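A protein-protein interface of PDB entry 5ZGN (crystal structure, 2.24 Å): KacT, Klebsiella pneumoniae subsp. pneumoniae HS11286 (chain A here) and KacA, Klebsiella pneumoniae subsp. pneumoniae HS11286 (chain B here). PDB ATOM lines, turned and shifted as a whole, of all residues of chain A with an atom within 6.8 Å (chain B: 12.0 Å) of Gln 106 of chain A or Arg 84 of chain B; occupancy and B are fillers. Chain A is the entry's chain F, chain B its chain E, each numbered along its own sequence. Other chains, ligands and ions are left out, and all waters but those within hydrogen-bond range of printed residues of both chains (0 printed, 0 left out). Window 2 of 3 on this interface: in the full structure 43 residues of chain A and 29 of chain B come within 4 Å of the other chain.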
ATOM      1  N   LEU A   5     -11.451   2.521   7.356  1.00  0.00           N
ATOM      2  CA  LEU A   5     -10.745   1.689   8.319  1.00  0.00           C
ATOM      3  C   LEU A   5     -10.453   2.465   9.597  1.00  0.00           C
ATOM      4  O   LEU A   5     -10.185   3.671   9.575  1.00  0.00           O
ATOM      5  CB  LEU A   5      -9.439   1.156   7.724  1.00  0.00           C
ATOM      6  CG  LEU A   5      -9.529   0.303   6.454  1.00  0.00           C
ATOM      7  CD1 LEU A   5      -8.192  -0.356   6.146  1.00  0.00           C
ATOM      8  CD2 LEU A   5     -10.623  -0.740   6.575  1.00  0.00           C
ATOM      9  N   SER A 102      -5.065  -7.931   1.067  1.00  0.00           N
ATOM     10  CA  SER A 102      -5.963  -7.010   0.374  1.00  0.00           C
ATOM     11  C   SER A 102      -5.539  -5.558   0.555  1.00  0.00           C
ATOM     12  O   SER A 102      -5.718  -4.746  -0.358  1.00  0.00           O
ATOM     13  CB  SER A 102      -7.403  -7.203   0.850  1.00  0.00           C
ATOM     14  OG  SER A 102      -7.531  -6.901   2.228  1.00  0.00           O
ATOM     15  N   VAL A 103      -4.991  -5.210   1.716  1.00  0.00           N
ATOM     16  CA  VAL A 103      -4.672  -3.826   2.046  1.00  0.00           C
ATOM     17  C   VAL A 103      -3.164  -3.618   2.208  1.00  0.00           C
ATOM     18  O   VAL A 103      -2.735  -2.666   2.860  1.00  0.00           O
ATOM     19  CB  VAL A 103      -5.440  -3.363   3.297  1.00  0.00           C
ATOM     20  CG1 VAL A 103      -6.923  -3.649   3.145  1.00  0.00           C
ATOM     21  CG2 VAL A 103      -4.911  -4.057   4.545  1.00  0.00           C
ATOM     22  N   GLN A 104      -2.350  -4.468   1.588  1.00  0.00           N
ATOM     23  CA  GLN A 104      -0.908  -4.305   1.680  1.00  0.00           C
ATOM     24  C   GLN A 104      -0.420  -3.286   0.654  1.00  0.00           C
ATOM     25  O   GLN A 104      -1.092  -2.987  -0.336  1.00  0.00           O
ATOM     26  CB  GLN A 104      -0.196  -5.643   1.478  1.00  0.00           C
ATOM     27  CG  GLN A 104      -0.174  -6.520   2.722  1.00  0.00           C
ATOM     28  CD  GLN A 104       0.617  -7.798   2.527  1.00  0.00           C
ATOM     29  OE1 GLN A 104       1.164  -8.045   1.452  1.00  0.00           O
ATOM     30  NE2 GLN A 104       0.684  -8.618   3.569  1.00  0.00           N
ATOM     31  N   GLY A 105       0.772  -2.749   0.908  1.00  0.00           N
ATOM     32  CA  GLY A 105       1.328  -1.746   0.024  1.00  0.00           C
ATOM     33  C   GLY A 105       0.584  -0.432   0.020  1.00  0.00           C
ATOM     34  O   GLY A 105       0.750   0.359  -0.911  1.00  0.00           O
ATOM     35  N   GLN A 106      -0.234  -0.169   1.038  1.00  0.00           N
ATOM     36  CA  GLN A 106      -0.996   1.071   1.108  1.00  0.00           C
ATOM     37  C   GLN A 106      -0.599   1.930   2.302  1.00  0.00           C
ATOM     38  O   GLN A 106      -1.181   3.004   2.498  1.00  0.00           O
ATOM     39  CB  GLN A 106      -2.500   0.781   1.163  1.00  0.00           C
ATOM     40  CG  GLN A 106      -3.031  -0.084   0.026  1.00  0.00           C
ATOM     41  CD  GLN A 106      -4.549  -0.194   0.029  1.00  0.00           C
ATOM     42  OE1 GLN A 106      -5.201   0.043   1.044  1.00  0.00           O
ATOM     43  NE2 GLN A 106      -5.111  -0.604  -1.093  1.00  0.00           N
ATOM     44  N   GLY A 107       0.382   1.499   3.093  1.00  0.00           N
ATOM     45  CA  GLY A 107       0.836   2.276   4.225  1.00  0.00           C
ATOM     46  C   GLY A 107       0.193   1.934   5.552  1.00  0.00           C
ATOM     47  O   GLY A 107       0.519   2.577   6.560  1.00  0.00           O
ATOM     48  N   TRP A 108      -0.721   0.960   5.591  1.00  0.00           N
ATOM     49  CA  TRP A 108      -1.365   0.611   6.854  1.00  0.00           C
ATOM     50  C   TRP A 108      -0.388  -0.030   7.828  1.00  0.00           C
ATOM     51  O   TRP A 108      -0.579   0.063   9.046  1.00  0.00           O
ATOM     52  CB  TRP A 108      -2.547  -0.325   6.613  1.00  0.00           C
ATOM     53  CG  TRP A 108      -3.555   0.209   5.655  1.00  0.00           C
ATOM     54  CD1 TRP A 108      -3.731  -0.175   4.364  1.00  0.00           C
ATOM     55  CD2 TRP A 108      -4.533   1.229   5.909  1.00  0.00           C
ATOM     56  NE1 TRP A 108      -4.754   0.535   3.795  1.00  0.00           N
ATOM     57  CE2 TRP A 108      -5.264   1.406   4.720  1.00  0.00           C
ATOM     58  CE3 TRP A 108      -4.859   2.006   7.022  1.00  0.00           C
ATOM     59  CZ2 TRP A 108      -6.302   2.329   4.610  1.00  0.00           C
ATOM     60  CZ3 TRP A 108      -5.891   2.921   6.913  1.00  0.00           C
ATOM     61  CH2 TRP A 108      -6.600   3.075   5.715  1.00  0.00           C
ATOM     62  N   GLY A 109       0.650  -0.695   7.318  1.00  0.00           N
ATOM     63  CA  GLY A 109       1.632  -1.294   8.206  1.00  0.00           C
ATOM     64  C   GLY A 109       2.379  -0.256   9.020  1.00  0.00           C
ATOM     65  O   GLY A 109       2.623  -0.443  10.214  1.00  0.00           O
ATOM     66  N   GLU A 110       2.743   0.860   8.384  1.00  0.00           N
ATOM     67  CA  GLU A 110       3.421   1.929   9.106  1.00  0.00           C
ATOM     68  C   GLU A 110       2.454   2.722   9.979  1.00  0.00           C
ATOM     69  O   GLU A 110       2.856   3.247  11.023  1.00  0.00           O
ATOM     70  CB  GLU A 110       4.124   2.859   8.118  1.00  0.00           C
ATOM     71  CG  GLU A 110       4.553   2.177   6.835  1.00  0.00           C
ATOM     72  CD  GLU A 110       5.485   3.035   6.002  1.00  0.00           C
ATOM     73  OE1 GLU A 110       5.051   4.113   5.542  1.00  0.00           O
ATOM     74  OE2 GLU A 110       6.648   2.629   5.813  1.00  0.00           O
ATOM     75  N   MET A 111       1.185   2.825   9.570  1.00  0.00           N
ATOM     76  CA  MET A 111       0.200   3.499  10.410  1.00  0.00           C
ATOM     77  C   MET A 111      -0.066   2.719  11.690  1.00  0.00           C
ATOM     78  O   MET A 111      -0.298   3.322  12.745  1.00  0.00           O
ATOM     79  CB  MET A 111      -1.106   3.702   9.645  1.00  0.00           C
ATOM     80  CG  MET A 111      -2.118   4.572  10.375  1.00  0.00           C
ATOM     81  SD  MET A 111      -3.580   4.949   9.387  1.00  0.00           S
ATOM     82  CE  MET A 111      -4.793   3.868  10.135  1.00  0.00           C
ATOM     83  N   LEU A 112      -0.038   1.388  11.616  1.00  0.00           N
ATOM     84  CA  LEU A 112      -0.139   0.582  12.826  1.00  0.00           C
ATOM     85  C   LEU A 112       1.058   0.820  13.738  1.00  0.00           C
ATOM     86  O   LEU A 112       0.900   0.966  14.955  1.00  0.00           O
ATOM     87  CB  LEU A 112      -0.266  -0.898  12.458  1.00  0.00           C
ATOM     88  CG  LEU A 112      -1.640  -1.318  11.922  1.00  0.00           C
ATOM     89  CD1 LEU A 112      -1.758  -2.822  11.812  1.00  0.00           C
ATOM     90  CD2 LEU A 112      -2.732  -0.791  12.827  1.00  0.00           C
ATOM     91  N   ASP A 175       3.099  16.896  15.506  1.00  0.00           N
ATOM     92  CA  ASP A 175       1.900  16.640  14.722  1.00  0.00           C
ATOM     93  C   ASP A 175       0.651  17.051  15.501  1.00  0.00           C
ATOM     94  O   ASP A 175       0.746  17.626  16.586  1.00  0.00           O
ATOM     95  CB  ASP A 175       1.835  15.161  14.335  1.00  0.00           C
ATOM     96  CG  ASP A 175       0.471  14.744  13.824  1.00  0.00           C
ATOM     97  OD1 ASP A 175      -0.190  15.544  13.128  1.00  0.00           O
ATOM     98  OD2 ASP A 175       0.063  13.603  14.123  1.00  0.00           O
ATOM     99  N   ASN B  75      12.074  10.591  11.220  1.00  0.00           N
ATOM    100  CA  ASN B  75      12.331  10.861   9.813  1.00  0.00           C
ATOM    101  C   ASN B  75      11.029  11.196   9.082  1.00  0.00           C
ATOM    102  O   ASN B  75       9.935  11.186   9.655  1.00  0.00           O
ATOM    103  CB  ASN B  75      13.068   9.681   9.174  1.00  0.00           C
ATOM    104  CG  ASN B  75      12.256   8.391   9.174  1.00  0.00           C
ATOM    105  OD1 ASN B  75      11.035   8.397   9.327  1.00  0.00           O
ATOM    106  ND2 ASN B  75      12.946   7.270   9.003  1.00  0.00           N
ATOM    107  N   ASP B  76      11.159  11.489   7.783  1.00  0.00           N
ATOM    108  CA  ASP B  76      10.014  11.939   6.998  1.00  0.00           C
ATOM    109  C   ASP B  76       8.970  10.840   6.845  1.00  0.00           C
ATOM    110  O   ASP B  76       7.765  11.110   6.908  1.00  0.00           O
ATOM    111  CB  ASP B  76      10.478  12.421   5.624  1.00  0.00           C
ATOM    112  CG  ASP B  76      11.252  13.720   5.694  1.00  0.00           C
ATOM    113  OD1 ASP B  76      11.423  14.250   6.812  1.00  0.00           O
ATOM    114  OD2 ASP B  76      11.679  14.216   4.631  1.00  0.00           O
ATOM    115  N   ARG B  77       9.407   9.597   6.640  1.00  0.00           N
ATOM    116  CA  ARG B  77       8.452   8.507   6.477  1.00  0.00           C
ATOM    117  C   ARG B  77       7.651   8.272   7.752  1.00  0.00           C
ATOM    118  O   ARG B  77       6.438   8.037   7.694  1.00  0.00           O
ATOM    119  CB  ARG B  77       9.172   7.224   6.067  1.00  0.00           C
ATOM    120  CG  ARG B  77       8.365   5.972   6.372  1.00  0.00           C
ATOM    121  CD  ARG B  77       8.965   4.725   5.757  1.00  0.00           C
ATOM    122  NE  ARG B  77       8.273   4.326   4.537  1.00  0.00           N
ATOM    123  CZ  ARG B  77       8.743   4.536   3.313  1.00  0.00           C
ATOM    124  NH1 ARG B  77       9.906   5.152   3.148  1.00  0.00           N
ATOM    125  NH2 ARG B  77       8.051   4.142   2.252  1.00  0.00           N
ATOM    126  N   LEU B  78       8.307   8.346   8.911  1.00  0.00           N
ATOM    127  CA  LEU B  78       7.607   8.072  10.160  1.00  0.00           C
ATOM    128  C   LEU B  78       6.596   9.164  10.497  1.00  0.00           C
ATOM    129  O   LEU B  78       5.467   8.858  10.903  1.00  0.00           O
ATOM    130  CB  LEU B  78       8.611   7.899  11.298  1.00  0.00           C
ATOM    131  CG  LEU B  78       7.960   7.651  12.653  1.00  0.00           C
ATOM    132  CD1 LEU B  78       7.057   6.441  12.526  1.00  0.00           C
ATOM    133  CD2 LEU B  78       9.005   7.437  13.732  1.00  0.00           C
ATOM    134  N   LYS B  79       6.970  10.440  10.342  1.00  0.00           N
ATOM    135  CA  LYS B  79       5.990  11.504  10.553  1.00  0.00           C
ATOM    136  C   LYS B  79       4.822  11.374   9.585  1.00  0.00           C
ATOM    137  O   LYS B  79       3.671  11.638   9.952  1.00  0.00           O
ATOM    138  CB  LYS B  79       6.623  12.893  10.435  1.00  0.00           C
ATOM    139  CG  LYS B  79       7.337  13.369  11.696  1.00  0.00           C
ATOM    140  CD  LYS B  79       7.911  14.773  11.529  1.00  0.00           C
ATOM    141  CE  LYS B  79       8.881  14.896  10.372  1.00  0.00           C
ATOM    142  NZ  LYS B  79       8.925  16.312   9.900  1.00  0.00           N
ATOM    143  N   ARG B  80       5.097  10.972   8.342  1.00  0.00           N
ATOM    144  CA  ARG B  80       4.027  10.819   7.361  1.00  0.00           C
ATOM    145  C   ARG B  80       3.042   9.732   7.777  1.00  0.00           C
ATOM    146  O   ARG B  80       1.843   9.842   7.491  1.00  0.00           O
ATOM    147  CB  ARG B  80       4.629  10.539   5.980  1.00  0.00           C
ATOM    148  CG  ARG B  80       3.620  10.420   4.845  1.00  0.00           C
ATOM    149  CD  ARG B  80       4.275  10.561   3.465  1.00  0.00           C
ATOM    150  NE  ARG B  80       5.507   9.797   3.304  1.00  0.00           N
ATOM    151  CZ  ARG B  80       6.726  10.336   3.305  1.00  0.00           C
ATOM    152  NH1 ARG B  80       6.881  11.645   3.463  1.00  0.00           N
ATOM    153  NH2 ARG B  80       7.795   9.563   3.144  1.00  0.00           N
ATOM    154  N   ALA B  81       3.518   8.682   8.454  1.00  0.00           N
ATOM    155  CA  ALA B  81       2.612   7.638   8.923  1.00  0.00           C
ATOM    156  C   ALA B  81       1.714   8.134  10.051  1.00  0.00           C
ATOM    157  O   ALA B  81       0.554   7.716  10.146  1.00  0.00           O
ATOM    158  CB  ALA B  81       3.403   6.410   9.374  1.00  0.00           C
ATOM    159  N   ALA B  82       2.225   9.016  10.912  1.00  0.00           N
ATOM    160  CA  ALA B  82       1.422   9.523  12.019  1.00  0.00           C
ATOM    161  C   ALA B  82       0.351  10.512  11.577  1.00  0.00           C
ATOM    162  O   ALA B  82      -0.619  10.715  12.313  1.00  0.00           O
ATOM    163  CB  ALA B  82       2.318  10.187  13.063  1.00  0.00           C
ATOM    164  N   LYS B  83       0.495  11.131  10.404  1.00  0.00           N
ATOM    165  CA  LYS B  83      -0.507  12.094   9.957  1.00  0.00           C
ATOM    166  C   LYS B  83      -1.744  11.390   9.420  1.00  0.00           C
ATOM    167  O   LYS B  83      -2.870  11.866   9.602  1.00  0.00           O
ATOM    168  CB  LYS B  83       0.090  12.982   8.874  1.00  0.00           C
ATOM    169  CG  LYS B  83       1.237  13.840   9.348  1.00  0.00           C
ATOM    170  CD  LYS B  83       2.295  13.916   8.264  1.00  0.00           C
ATOM    171  CE  LYS B  83       3.433  14.844   8.634  1.00  0.00           C
ATOM    172  NZ  LYS B  83       4.418  14.919   7.522  1.00  0.00           N
ATOM    173  N   ARG B  84      -1.549  10.239   8.768  1.00  0.00           N
ATOM    174  CA  ARG B  84      -2.676   9.422   8.338  1.00  0.00           C
ATOM    175  C   ARG B  84      -3.386   8.801   9.529  1.00  0.00           C
ATOM    176  O   ARG B  84      -4.590   8.527   9.462  1.00  0.00           O
ATOM    177  CB  ARG B  84      -2.196   8.330   7.388  1.00  0.00           C
ATOM    178  CG  ARG B  84      -1.328   8.798   6.225  1.00  0.00           C
ATOM    179  CD  ARG B  84      -0.486   7.650   5.672  1.00  0.00           C
ATOM    180  NE  ARG B  84      -1.281   6.553   5.133  1.00  0.00           N
ATOM    181  CZ  ARG B  84      -1.612   5.470   5.831  1.00  0.00           C
ATOM    182  NH1 ARG B  84      -1.214   5.353   7.088  1.00  0.00           N
ATOM    183  NH2 ARG B  84      -2.338   4.507   5.278  1.00  0.00           N
ATOM    184  N   LEU B  85      -2.654   8.573  10.622  1.00  0.00           N
ATOM    185  CA  LEU B  85      -3.281   8.100  11.847  1.00  0.00           C
ATOM    186  C   LEU B  85      -4.195   9.164  12.438  1.00  0.00           C
ATOM    187  O   LEU B  85      -5.235   8.836  13.021  1.00  0.00           O
ATOM    188  CB  LEU B  85      -2.208   7.691  12.855  1.00  0.00           C
ATOM    189  CG  LEU B  85      -2.722   7.134  14.181  1.00  0.00           C
ATOM    190  CD1 LEU B  85      -3.548   5.881  13.933  1.00  0.00           C
ATOM    191  CD2 LEU B  85      -1.569   6.851  15.131  1.00  0.00           C
ATOM    192  N   GLN B  86      -3.815  10.414  12.233  1.00  0.00           N
ATOM    193  CA  GLN B  86      -4.547  11.551  12.744  1.00  0.00           C
ATOM    194  C   GLN B  86      -5.393  12.232  11.687  1.00  0.00           C
ATOM    195  O   GLN B  86      -5.638  11.687  10.622  1.00  0.00           O
ATOM    196  CB  GLN B  86      -3.558  12.548  13.329  1.00  0.00           C
ATOM    197  CG  GLN B  86      -3.605  12.664  14.841  1.00  0.00           C
ATOM    198  CD  GLN B  86      -2.742  11.646  15.550  1.00  0.00           C
ATOM    199  OE1 GLN B  86      -1.675  11.301  15.080  1.00  0.00           O
ATOM    200  NE2 GLN B  86      -3.200  11.177  16.694  1.00  0.00           N
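The side-chain carboxylate of Glu 110 of chain A is in salt-bridge range of the guanidinium group of Arg 77 of chain B.
The backbone carbonyl oxygen of Gln 106 of chain A sits at hydrogen-bond distance from the guanidinium group of Arg 84 of chain B (3.4 Å).
The guanidinium group (NH1) of Arg 84 of chain B sits at hydrogen-bond distance from the backbone carbonyl oxygen (O) of Gly 107 of chain A (3.3 Å).
The guanidinium group of Arg 84 of chain B lies close to the side-chain sulfur of Met 111 of chain A.
OE1 of Gln 86 of chain B sits close to OD2 of Asp 175 of chain A (3.0 Å).
The side-chain carboxylate (OD2) of Asp 175 of chain A sits close to the backbone carbonyl oxygen (O) of Ala 82 of chain B.
The side-chain amide oxygen (OD1) of Asn 75 of chain B sits close to the backbone NH (N) of Arg 77 of chain B.
The backbone carbonyl oxygen (O) of Ala 82 of chain B sits close to the side-chain amide oxygen (OE1) of Gln 86 of chain B, 3.0 Å away.
NE1 of Trp 108 of chain A lies within hydrogen-bond range of OE1 of Gln 106 of chain A.
Among the printed residues, pairs that only touch across the chains: Trp 108 of chain A with Arg 84 of chain B (3.9 Å), Glu 110 of chain A with Ala 81 of chain B (3.6 Å) and Met 111 of chain A with Leu 85 of chain B (3.9 Å).
Gln 106 of chain A touches just one residue of chain B: Arg 84.
No residue of chain B comes within 4 Å of Ser 102 of chain A.
No residue of chain B comes within 4 Å of Val 103 of chain A.
Gly 105 of chain A touches none of the printed residues of chain B.
Of chain B, only Arg 84 (3.9 Å) comes within 4 Å of Trp 108 of chain A.
Met 111 of chain A touches just these residues of chain B: Arg 84 (3.0 Å) and Leu 85 (3.9 Å).
Of the printed residues of chain A, Gln 86 of chain B touches Asp 175 (3.0 Å).
Printed residues of chain A within 4 Å of Leu 85 of chain B: Met 111 (3.9 Å).
Printed residues of chain B within 4 Å of Glu 110 of chain A: Arg 77 and Ala 81.
The nearest residue of chain A that does not touch Arg 84 of chain B is Glu 110 of chain A (5.4 Å).
Printed residues of chain B that touch a printed residue of chain A: Arg 77, Ala 81, Ala 82, Arg 84, Leu 85 and Gln 86.
Along chain B the printed residues that touch a printed residue of chain A span positions 77 to 86.
Of the 13 printed residues of chain A, 6 touch a printed residue of chain B.
Hydrophobic or aromatic side chains of chain A within 4 Å of the printed part of chain B: Trp 108 and Met 111.
Among the printed residues, Asp or Glu carboxylates within 4 Å of a Lys or Arg side-chain nitrogen of the other chain: Glu 110 of chain A with Arg 77 of chain B (2.7 Å).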
